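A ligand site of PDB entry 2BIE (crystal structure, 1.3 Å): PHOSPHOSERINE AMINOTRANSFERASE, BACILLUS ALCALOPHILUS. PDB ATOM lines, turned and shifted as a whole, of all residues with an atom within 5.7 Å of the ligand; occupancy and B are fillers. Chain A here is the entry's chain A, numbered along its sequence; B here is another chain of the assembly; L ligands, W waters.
The side-chain carboxylate (OD1) of Asp 173 lies within hydrogen-bond range of the side-chain hydroxyl (OG) of Ser 175, at 2.7 Å.
The backbone NH of Gly 194 sits at hydrogen-bond distance from the side-chain hydroxyl of Ser 175, 3.4 Å away.
The backbone carbonyl oxygen of Thr 239 of chain B lies within hydrogen-bond range of the side-chain amide nitrogen of Gln 74 of chain B.
The side-chain hydroxyl (OG1) of Thr 153 sits at hydrogen-bond distance from the side-chain hydroxyl (OG) of Ser 176 (2.7 Å).
The side-chain amide nitrogen (ND2) of Asn 238 of chain B lies within hydrogen-bond range of the backbone carbonyl oxygen (O) of Gly 75 (3.1 Å).
The backbone NH of Gly 76 sits close to the side-chain hydroxyl of Thr 205 (3.1 Å).
The side-chain amide nitrogen (ND2) of Asn 151 is in hydrogen-bond range of the side-chain hydroxyl (OG) of Ser 176.
OG1 of Thr 239 of chain B sits at hydrogen-bond distance from NE2 of Gln 196 (3.2 Å).
Residues that only touch the ligand: Gly 76 (3.2 Å), Trp 103 (3.4 Å), Ser 175 (3.6 Å), Phe 81 (3.8 Å), Asn 151 (3.8 Å), Ser 176 (3.8 Å) and Thr 149 (3.9 Å).
Of the 23 residues printed, 15 come within 4 Å of the ligand.
Along chain A the residues within 4 Å of the ligand span positions 76 to 197.
Water W1 lies within hydrogen-bond range of O of Thr 239 of chain B, O5 of the ligand and NE2 of Gln 74 of chain B.
Water W2 lies within hydrogen-bond range of O2 of the ligand, OG of Ser 175 and N of Gly 194.
Water W5 lies within hydrogen-bond range of O of Asn 151 (2.9 Å), O of Asp 173 (3.0 Å), N of Ser 176 (3.1 Å) and N of Ser 175 (3.3 Å).
An oxygen (O5) of the ligand lies within hydrogen-bond range of the side-chain amide nitrogen (NE2) of Gln 196 (2.9 Å).
ND2 of Asn 238 of chain B lies within hydrogen-bond range of O4 of the ligand (3.0 Å).
The side-chain carboxylate of Asp 173 lies within hydrogen-bond range of a nitrogen (N1) of the ligand (2.7 Å).
The side-chain hydroxyl of Thr 153 lies within hydrogen-bond range of an oxygen (O1) of the ligand (2.5 Å).
An oxygen (O4) of the ligand lies within hydrogen-bond range of the backbone NH of Ser 78, at 2.8 Å.
OG of Ser 78 sits at hydrogen-bond distance from O4 of the ligand (2.6 Å).
The side-chain amino group (NZ) of Lys 197 is bonded to a carbon (C5) of the ligand.
An oxygen (O3) of the ligand is in hydrogen-bond range of the side-chain hydroxyl (OG1) of Thr 239 of chain B (2.7 Å).
An oxygen (O3) of the ligand lies within hydrogen-bond range of the backbone NH of Thr 239 of chain B (2.9 Å).
An oxygen (O5) of the ligand lies within hydrogen-bond range of the backbone NH (N) of Ala 77, at 3.2 Å.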
ATOM      1  N   GLY A  75     -11.668  15.940   8.099  1.00  0.00           N
ATOM      2  CA  GLY A  75     -12.270  15.464   9.322  1.00  0.00           C
ATOM      3  C   GLY A  75     -13.775  15.524   9.407  1.00  0.00           C
ATOM      4  O   GLY A  75     -14.370  14.978  10.333  1.00  0.00           O
ATOM      5  N   GLY A  76     -14.391  16.215   8.430  1.00  0.00           N
ATOM      6  CA  GLY A  76     -15.829  16.371   8.447  1.00  0.00           C
ATOM      7  C   GLY A  76     -16.299  17.457   9.374  1.00  0.00           C
ATOM      8  O   GLY A  76     -15.562  18.000  10.172  1.00  0.00           O
ATOM      9  N   ALA A  77     -17.604  17.757   9.256  1.00  0.00           N
ATOM     10  CA  ALA A  77     -18.195  18.616  10.294  1.00  0.00           C
ATOM     11  C   ALA A  77     -18.037  18.017  11.669  1.00  0.00           C
ATOM     12  O   ALA A  77     -17.931  18.772  12.656  1.00  0.00           O
ATOM     13  CB  ALA A  77     -19.663  18.897   9.951  1.00  0.00           C
ATOM     14  N   SER A  78     -18.026  16.687  11.749  1.00  0.00           N
ATOM     15  CA  SER A  78     -17.925  16.088  13.090  1.00  0.00           C
ATOM     16  C   SER A  78     -16.634  16.472  13.794  1.00  0.00           C
ATOM     17  O   SER A  78     -16.613  16.617  15.006  1.00  0.00           O
ATOM     18  CB  SER A  78     -18.018  14.565  13.019  1.00  0.00           C
ATOM     19  OG  SER A  78     -19.275  14.154  12.507  1.00  0.00           O
ATOM     20  N   LEU A  79     -15.515  16.625  13.042  1.00  0.00           N
ATOM     21  CA  LEU A  79     -14.314  17.065  13.732  1.00  0.00           C
ATOM     22  C   LEU A  79     -14.445  18.490  14.201  1.00  0.00           C
ATOM     23  O   LEU A  79     -13.864  18.860  15.240  1.00  0.00           O
ATOM     24  CB  LEU A  79     -13.043  16.898  12.842  1.00  0.00           C
ATOM     25  CG  LEU A  79     -11.743  17.138  13.607  1.00  0.00           C
ATOM     26  CD1 LEU A  79     -11.519  16.150  14.738  1.00  0.00           C
ATOM     27  CD2 LEU A  79     -10.574  17.073  12.647  1.00  0.00           C
ATOM     28  N   PHE A  81     -17.019  19.735  15.502  1.00  0.00           N
ATOM     29  CA  PHE A  81     -17.753  19.737  16.772  1.00  0.00           C
ATOM     30  C   PHE A  81     -16.774  19.757  17.953  1.00  0.00           C
ATOM     31  O   PHE A  81     -17.119  20.353  18.959  1.00  0.00           O
ATOM     32  CB  PHE A  81     -18.637  18.520  16.936  1.00  0.00           C
ATOM     33  CG  PHE A  81     -19.764  18.326  15.932  1.00  0.00           C
ATOM     34  CD1 PHE A  81     -20.329  17.075  15.747  1.00  0.00           C
ATOM     35  CD2 PHE A  81     -20.249  19.389  15.190  1.00  0.00           C
ATOM     36  CE1 PHE A  81     -21.394  16.868  14.906  1.00  0.00           C
ATOM     37  CE2 PHE A  81     -21.334  19.211  14.335  1.00  0.00           C
ATOM     38  CZ  PHE A  81     -21.878  17.966  14.207  1.00  0.00           C
ATOM     39  N   TRP A 103     -28.120  16.736  14.892  1.00  0.00           N
ATOM     40  CA  TRP A 103     -26.770  17.291  14.673  1.00  0.00           C
ATOM     41  C   TRP A 103     -26.426  18.375  15.683  1.00  0.00           C
ATOM     42  O   TRP A 103     -25.278  18.491  16.107  1.00  0.00           O
ATOM     43  CB  TRP A 103     -26.655  17.800  13.228  1.00  0.00           C
ATOM     44  CG  TRP A 103     -26.612  16.651  12.234  1.00  0.00           C
ATOM     45  CD1 TRP A 103     -27.522  16.373  11.247  1.00  0.00           C
ATOM     46  CD2 TRP A 103     -25.619  15.651  12.165  1.00  0.00           C
ATOM     47  NE1 TRP A 103     -27.127  15.228  10.549  1.00  0.00           N
ATOM     48  CE2 TRP A 103     -25.976  14.790  11.096  1.00  0.00           C
ATOM     49  CE3 TRP A 103     -24.449  15.420  12.909  1.00  0.00           C
ATOM     50  CZ2 TRP A 103     -25.191  13.705  10.766  1.00  0.00           C
ATOM     51  CZ3 TRP A 103     -23.671  14.323  12.562  1.00  0.00           C
ATOM     52  CH2 TRP A 103     -24.055  13.487  11.509  1.00  0.00           C
ATOM     53  N   THR A 149     -27.412  25.250  14.301  1.00  0.00           N
ATOM     54  CA  THR A 149     -27.368  24.334  13.167  1.00  0.00           C
ATOM     55  C   THR A 149     -28.355  24.922  12.189  1.00  0.00           C
ATOM     56  O   THR A 149     -29.575  24.879  12.432  1.00  0.00           O
ATOM     57  CB  THR A 149     -27.799  22.933  13.603  1.00  0.00           C
ATOM     58  OG1 THR A 149     -27.046  22.551  14.765  1.00  0.00           O
ATOM     59  CG2 THR A 149     -27.573  21.929  12.463  1.00  0.00           C
ATOM     60  N   ASN A 151     -29.542  24.171   9.146  1.00  0.00           N
ATOM     61  CA  ASN A 151     -30.441  23.237   8.509  1.00  0.00           C
ATOM     62  C   ASN A 151     -30.291  21.915   9.248  1.00  0.00           C
ATOM     63  O   ASN A 151     -29.215  21.330   9.318  1.00  0.00           O
ATOM     64  CB  ASN A 151     -30.156  23.119   7.007  1.00  0.00           C
ATOM     65  CG  ASN A 151     -31.235  22.286   6.310  1.00  0.00           C
ATOM     66  OD1 ASN A 151     -32.333  22.840   6.040  1.00  0.00           O
ATOM     67  ND2 ASN A 151     -30.937  21.026   6.040  1.00  0.00           N
ATOM     68  N   ASN A 152     -31.392  21.458   9.843  1.00  0.00           N
ATOM     69  CA  ASN A 152     -31.400  20.273  10.667  1.00  0.00           C
ATOM     70  C   ASN A 152     -31.769  19.086   9.767  1.00  0.00           C
ATOM     71  O   ASN A 152     -32.918  18.749   9.563  1.00  0.00           O
ATOM     72  CB  ASN A 152     -32.389  20.461  11.822  1.00  0.00           C
ATOM     73  CG  ASN A 152     -32.017  21.721  12.556  1.00  0.00           C
ATOM     74  OD1 ASN A 152     -31.037  21.702  13.335  1.00  0.00           O
ATOM     75  ND2 ASN A 152     -32.779  22.802  12.338  1.00  0.00           N
ATOM     76  N   THR A 153     -30.691  18.468   9.249  1.00  0.00           N
ATOM     77  CA  THR A 153     -30.759  17.572   8.119  1.00  0.00           C
ATOM     78  C   THR A 153     -31.677  16.382   8.363  1.00  0.00           C
ATOM     79  O   THR A 153     -32.327  15.870   7.447  1.00  0.00           O
ATOM     80  CB  THR A 153     -29.318  17.033   7.846  1.00  0.00           C
ATOM     81  OG1 THR A 153     -28.412  18.124   8.071  1.00  0.00           O
ATOM     82  CG2 THR A 153     -29.138  16.535   6.423  1.00  0.00           C
ATOM     83  N   ASP A 173     -23.168  25.369  12.142  1.00  0.00           N
ATOM     84  CA  ASP A 173     -23.029  24.162  11.337  1.00  0.00           C
ATOM     85  C   ASP A 173     -23.988  24.304  10.152  1.00  0.00           C
ATOM     86  O   ASP A 173     -25.191  24.115  10.357  1.00  0.00           O
ATOM     87  CB  ASP A 173     -23.335  22.940  12.196  1.00  0.00           C
ATOM     88  CG  ASP A 173     -23.297  21.671  11.406  1.00  0.00           C
ATOM     89  OD1 ASP A 173     -23.038  21.659  10.181  1.00  0.00           O
ATOM     90  OD2 ASP A 173     -23.541  20.615  12.060  1.00  0.00           O
ATOM     91  N   MET A 174     -23.475  24.681   9.011  1.00  0.00           N
ATOM     92  CA  MET A 174     -24.262  24.899   7.817  1.00  0.00           C
ATOM     93  C   MET A 174     -24.056  23.764   6.817  1.00  0.00           C
ATOM     94  O   MET A 174     -24.270  23.991   5.613  1.00  0.00           O
ATOM     95  CB  MET A 174     -23.946  26.227   7.171  1.00  0.00           C
ATOM     96  CG  MET A 174     -24.256  27.429   8.075  1.00  0.00           C
ATOM     97  SD  MET A 174     -24.222  28.943   7.151  1.00  0.00           S
ATOM     98  CE  MET A 174     -24.788  30.131   8.362  1.00  0.00           C
ATOM     99  N   SER A 175     -23.658  22.608   7.311  1.00  0.00           N
ATOM    100  CA  SER A 175     -23.374  21.489   6.414  1.00  0.00           C
ATOM    101  C   SER A 175     -24.453  21.261   5.337  1.00  0.00           C
ATOM    102  O   SER A 175     -24.065  21.073   4.186  1.00  0.00           O
ATOM    103  CB  SER A 175     -23.230  20.198   7.192  1.00  0.00           C
ATOM    104  OG  SER A 175     -22.121  20.237   8.066  1.00  0.00           O
ATOM    105  N   SER A 176     -25.727  21.283   5.691  1.00  0.00           N
ATOM    106  CA  SER A 176     -26.707  20.849   4.730  1.00  0.00           C
ATOM    107  C   SER A 176     -27.401  21.995   4.017  1.00  0.00           C
ATOM    108  O   SER A 176     -28.291  21.714   3.204  1.00  0.00           O
ATOM    109  CB  SER A 176     -27.671  19.834   5.369  1.00  0.00           C
ATOM    110  OG  SER A 176     -28.210  20.362   6.587  1.00  0.00           O
ATOM    111  N   GLY A 194     -19.339  20.263   6.122  1.00  0.00           N
ATOM    112  CA  GLY A 194     -18.798  19.204   5.280  1.00  0.00           C
ATOM    113  C   GLY A 194     -19.229  19.471   3.877  1.00  0.00           C
ATOM    114  O   GLY A 194     -20.397  19.845   3.633  1.00  0.00           O
ATOM    115  N   GLN A 196     -19.970  17.531   1.433  1.00  0.00           N
ATOM    116  CA  GLN A 196     -20.647  16.463   0.717  1.00  0.00           C
ATOM    117  C   GLN A 196     -22.171  16.595   0.683  1.00  0.00           C
ATOM    118  O   GLN A 196     -22.844  15.679   0.223  1.00  0.00           O
ATOM    119  CB  GLN A 196     -20.327  15.120   1.342  1.00  0.00           C
ATOM    120  CG  GLN A 196     -20.822  14.905   2.752  1.00  0.00           C
ATOM    121  CD  GLN A 196     -19.877  15.361   3.868  1.00  0.00           C
ATOM    122  OE1 GLN A 196     -18.896  16.077   3.593  1.00  0.00           O
ATOM    123  NE2 GLN A 196     -20.172  14.936   5.088  1.00  0.00           N
ATOM    124  N   LYS A 197     -22.738  17.678   1.199  1.00  0.00           N
ATOM    125  CA  LYS A 197     -24.197  17.814   1.061  1.00  0.00           C
ATOM    126  C   LYS A 197     -24.514  18.767  -0.086  1.00  0.00           C
ATOM    127  O   LYS A 197     -25.201  18.402  -1.027  1.00  0.00           O
ATOM    128  CB  LYS A 197     -24.904  18.217   2.355  1.00  0.00           C
ATOM    129  CG  LYS A 197     -24.407  17.593   3.652  1.00  0.00           C
ATOM    130  CD  LYS A 197     -25.245  16.504   4.219  1.00  0.00           C
ATOM    131  CE  LYS A 197     -24.568  15.503   5.098  1.00  0.00           C
ATOM    132  NZ  LYS A 197     -24.710  15.878   6.528  1.00  0.00           N
ATOM    133  N   THR A 205     -13.934  19.826   4.442  1.00  0.00           N
ATOM    134  CA  THR A 205     -14.845  20.623   5.274  1.00  0.00           C
ATOM    135  C   THR A 205     -14.462  22.075   5.043  1.00  0.00           C
ATOM    136  O   THR A 205     -13.290  22.445   5.210  1.00  0.00           O
ATOM    137  CB  THR A 205     -14.702  20.205   6.732  1.00  0.00           C
ATOM    138  OG1 THR A 205     -15.033  18.807   6.838  1.00  0.00           O
ATOM    139  CG2 THR A 205     -15.644  20.936   7.672  1.00  0.00           C
ATOM    140  N   TYR A 339     -30.862  19.075  -2.246  1.00  0.00           N
ATOM    141  CA  TYR A 339     -29.755  20.009  -2.290  1.00  0.00           C
ATOM    142  C   TYR A 339     -29.628  20.656  -3.656  1.00  0.00           C
ATOM    143  O   TYR A 339     -30.303  20.239  -4.646  1.00  0.00           O
ATOM    144  CB  TYR A 339     -28.496  19.191  -1.958  1.00  0.00           C
ATOM    145  CG  TYR A 339     -28.497  18.486  -0.658  1.00  0.00           C
ATOM    146  CD1 TYR A 339     -28.274  17.133  -0.565  1.00  0.00           C
ATOM    147  CD2 TYR A 339     -28.705  19.173   0.535  1.00  0.00           C
ATOM    148  CE1 TYR A 339     -28.261  16.429   0.608  1.00  0.00           C
ATOM    149  CE2 TYR A 339     -28.698  18.490   1.718  1.00  0.00           C
ATOM    150  CZ  TYR A 339     -28.475  17.127   1.766  1.00  0.00           C
ATOM    151  OH  TYR A 339     -28.487  16.519   3.025  1.00  0.00           O
ATOM    152  N   GLN B  74      -9.562  10.433   8.216  1.00  0.00           N
ATOM    153  CA  GLN B  74      -9.149  11.713   7.642  1.00  0.00           C
ATOM    154  C   GLN B  74      -8.076  12.366   8.499  1.00  0.00           C
ATOM    155  O   GLN B  74      -7.882  11.982   9.648  1.00  0.00           O
ATOM    156  CB  GLN B  74     -10.348  12.631   7.536  1.00  0.00           C
ATOM    157  CG  GLN B  74     -11.468  12.047   6.652  1.00  0.00           C
ATOM    158  CD  GLN B  74     -12.572  13.071   6.506  1.00  0.00           C
ATOM    159  OE1 GLN B  74     -12.335  14.170   5.971  1.00  0.00           O
ATOM    160  NE2 GLN B  74     -13.781  12.751   6.995  1.00  0.00           N
ATOM    161  N   ASN B 238     -18.537   8.814  11.032  1.00  0.00           N
ATOM    162  CA  ASN B 238     -18.996   9.975  10.237  1.00  0.00           C
ATOM    163  C   ASN B 238     -18.717   9.670   8.757  1.00  0.00           C
ATOM    164  O   ASN B 238     -18.343   8.550   8.410  1.00  0.00           O
ATOM    165  CB  ASN B 238     -18.416  11.298  10.691  1.00  0.00           C
ATOM    166  CG  ASN B 238     -16.936  11.506  10.330  1.00  0.00           C
ATOM    167  OD1 ASN B 238     -16.168  10.550  10.304  1.00  0.00           O
ATOM    168  ND2 ASN B 238     -16.601  12.794  10.085  1.00  0.00           N
ATOM    169  N   THR B 239     -18.941  10.683   7.931  1.00  0.00           N
ATOM    170  CA  THR B 239     -18.797  10.388   6.473  1.00  0.00           C
ATOM    171  C   THR B 239     -17.330  10.205   6.134  1.00  0.00           C
ATOM    172  O   THR B 239     -16.515  11.103   6.369  1.00  0.00           O
ATOM    173  CB  THR B 239     -19.377  11.550   5.673  1.00  0.00           C
ATOM    174  OG1 THR B 239     -20.682  11.930   6.122  1.00  0.00           O
ATOM    175  CG2 THR B 239     -19.490  11.157   4.208  1.00  0.00           C
HETATM  176  N1  LIG L   1     -23.836  18.386  10.640  1.00  0.00           N
HETATM  177  C1  LIG L   1     -24.879  18.406   9.781  1.00  0.00           C
HETATM  178  C2  LIG L   1     -25.947  19.490   9.937  1.00  0.00           C
HETATM  179  C3  LIG L   1     -24.942  17.457   8.793  1.00  0.00           C
HETATM  180  O1  LIG L   1     -25.970  17.517   7.920  1.00  0.00           O
HETATM  181  C4  LIG L   1     -23.920  16.512   8.680  1.00  0.00           C
HETATM  182  C5  LIG L   1     -23.751  15.702   7.396  1.00  0.00           C
HETATM  183  C6  LIG L   1     -22.914  16.445   9.641  1.00  0.00           C
HETATM  184  C7  LIG L   1     -22.900  17.408  10.628  1.00  0.00           C
HETATM  185  C8  LIG L   1     -21.863  15.324   9.694  1.00  0.00           C
HETATM  186  O2  LIG L   1     -20.822  15.634   8.766  1.00  0.00           O
HETATM  187  P1  LIG L   1     -19.561  14.647   8.645  1.00  0.00           P
HETATM  188  O3  LIG L   1     -20.079  13.294   8.349  1.00  0.00           O
HETATM  189  O4  LIG L   1     -18.864  14.703   9.985  1.00  0.00           O
HETATM  190  O5  LIG L   1     -18.722  15.250   7.560  1.00  0.00           O
HETATM  191  O   HOH W   1     -16.567  13.795   6.635  1.00  0.00           O
HETATM  192  O   HOH W   2     -21.047  17.781   7.003  1.00  0.00           O
HETATM  193  O   HOH W   3     -21.923  11.659   9.598  1.00  0.00           O
HETATM  194  O   HOH W   4     -24.359  12.542   7.219  1.00  0.00           O
HETATM  195  O   HOH W   5     -26.765  22.503   8.367  1.00  0.00           O
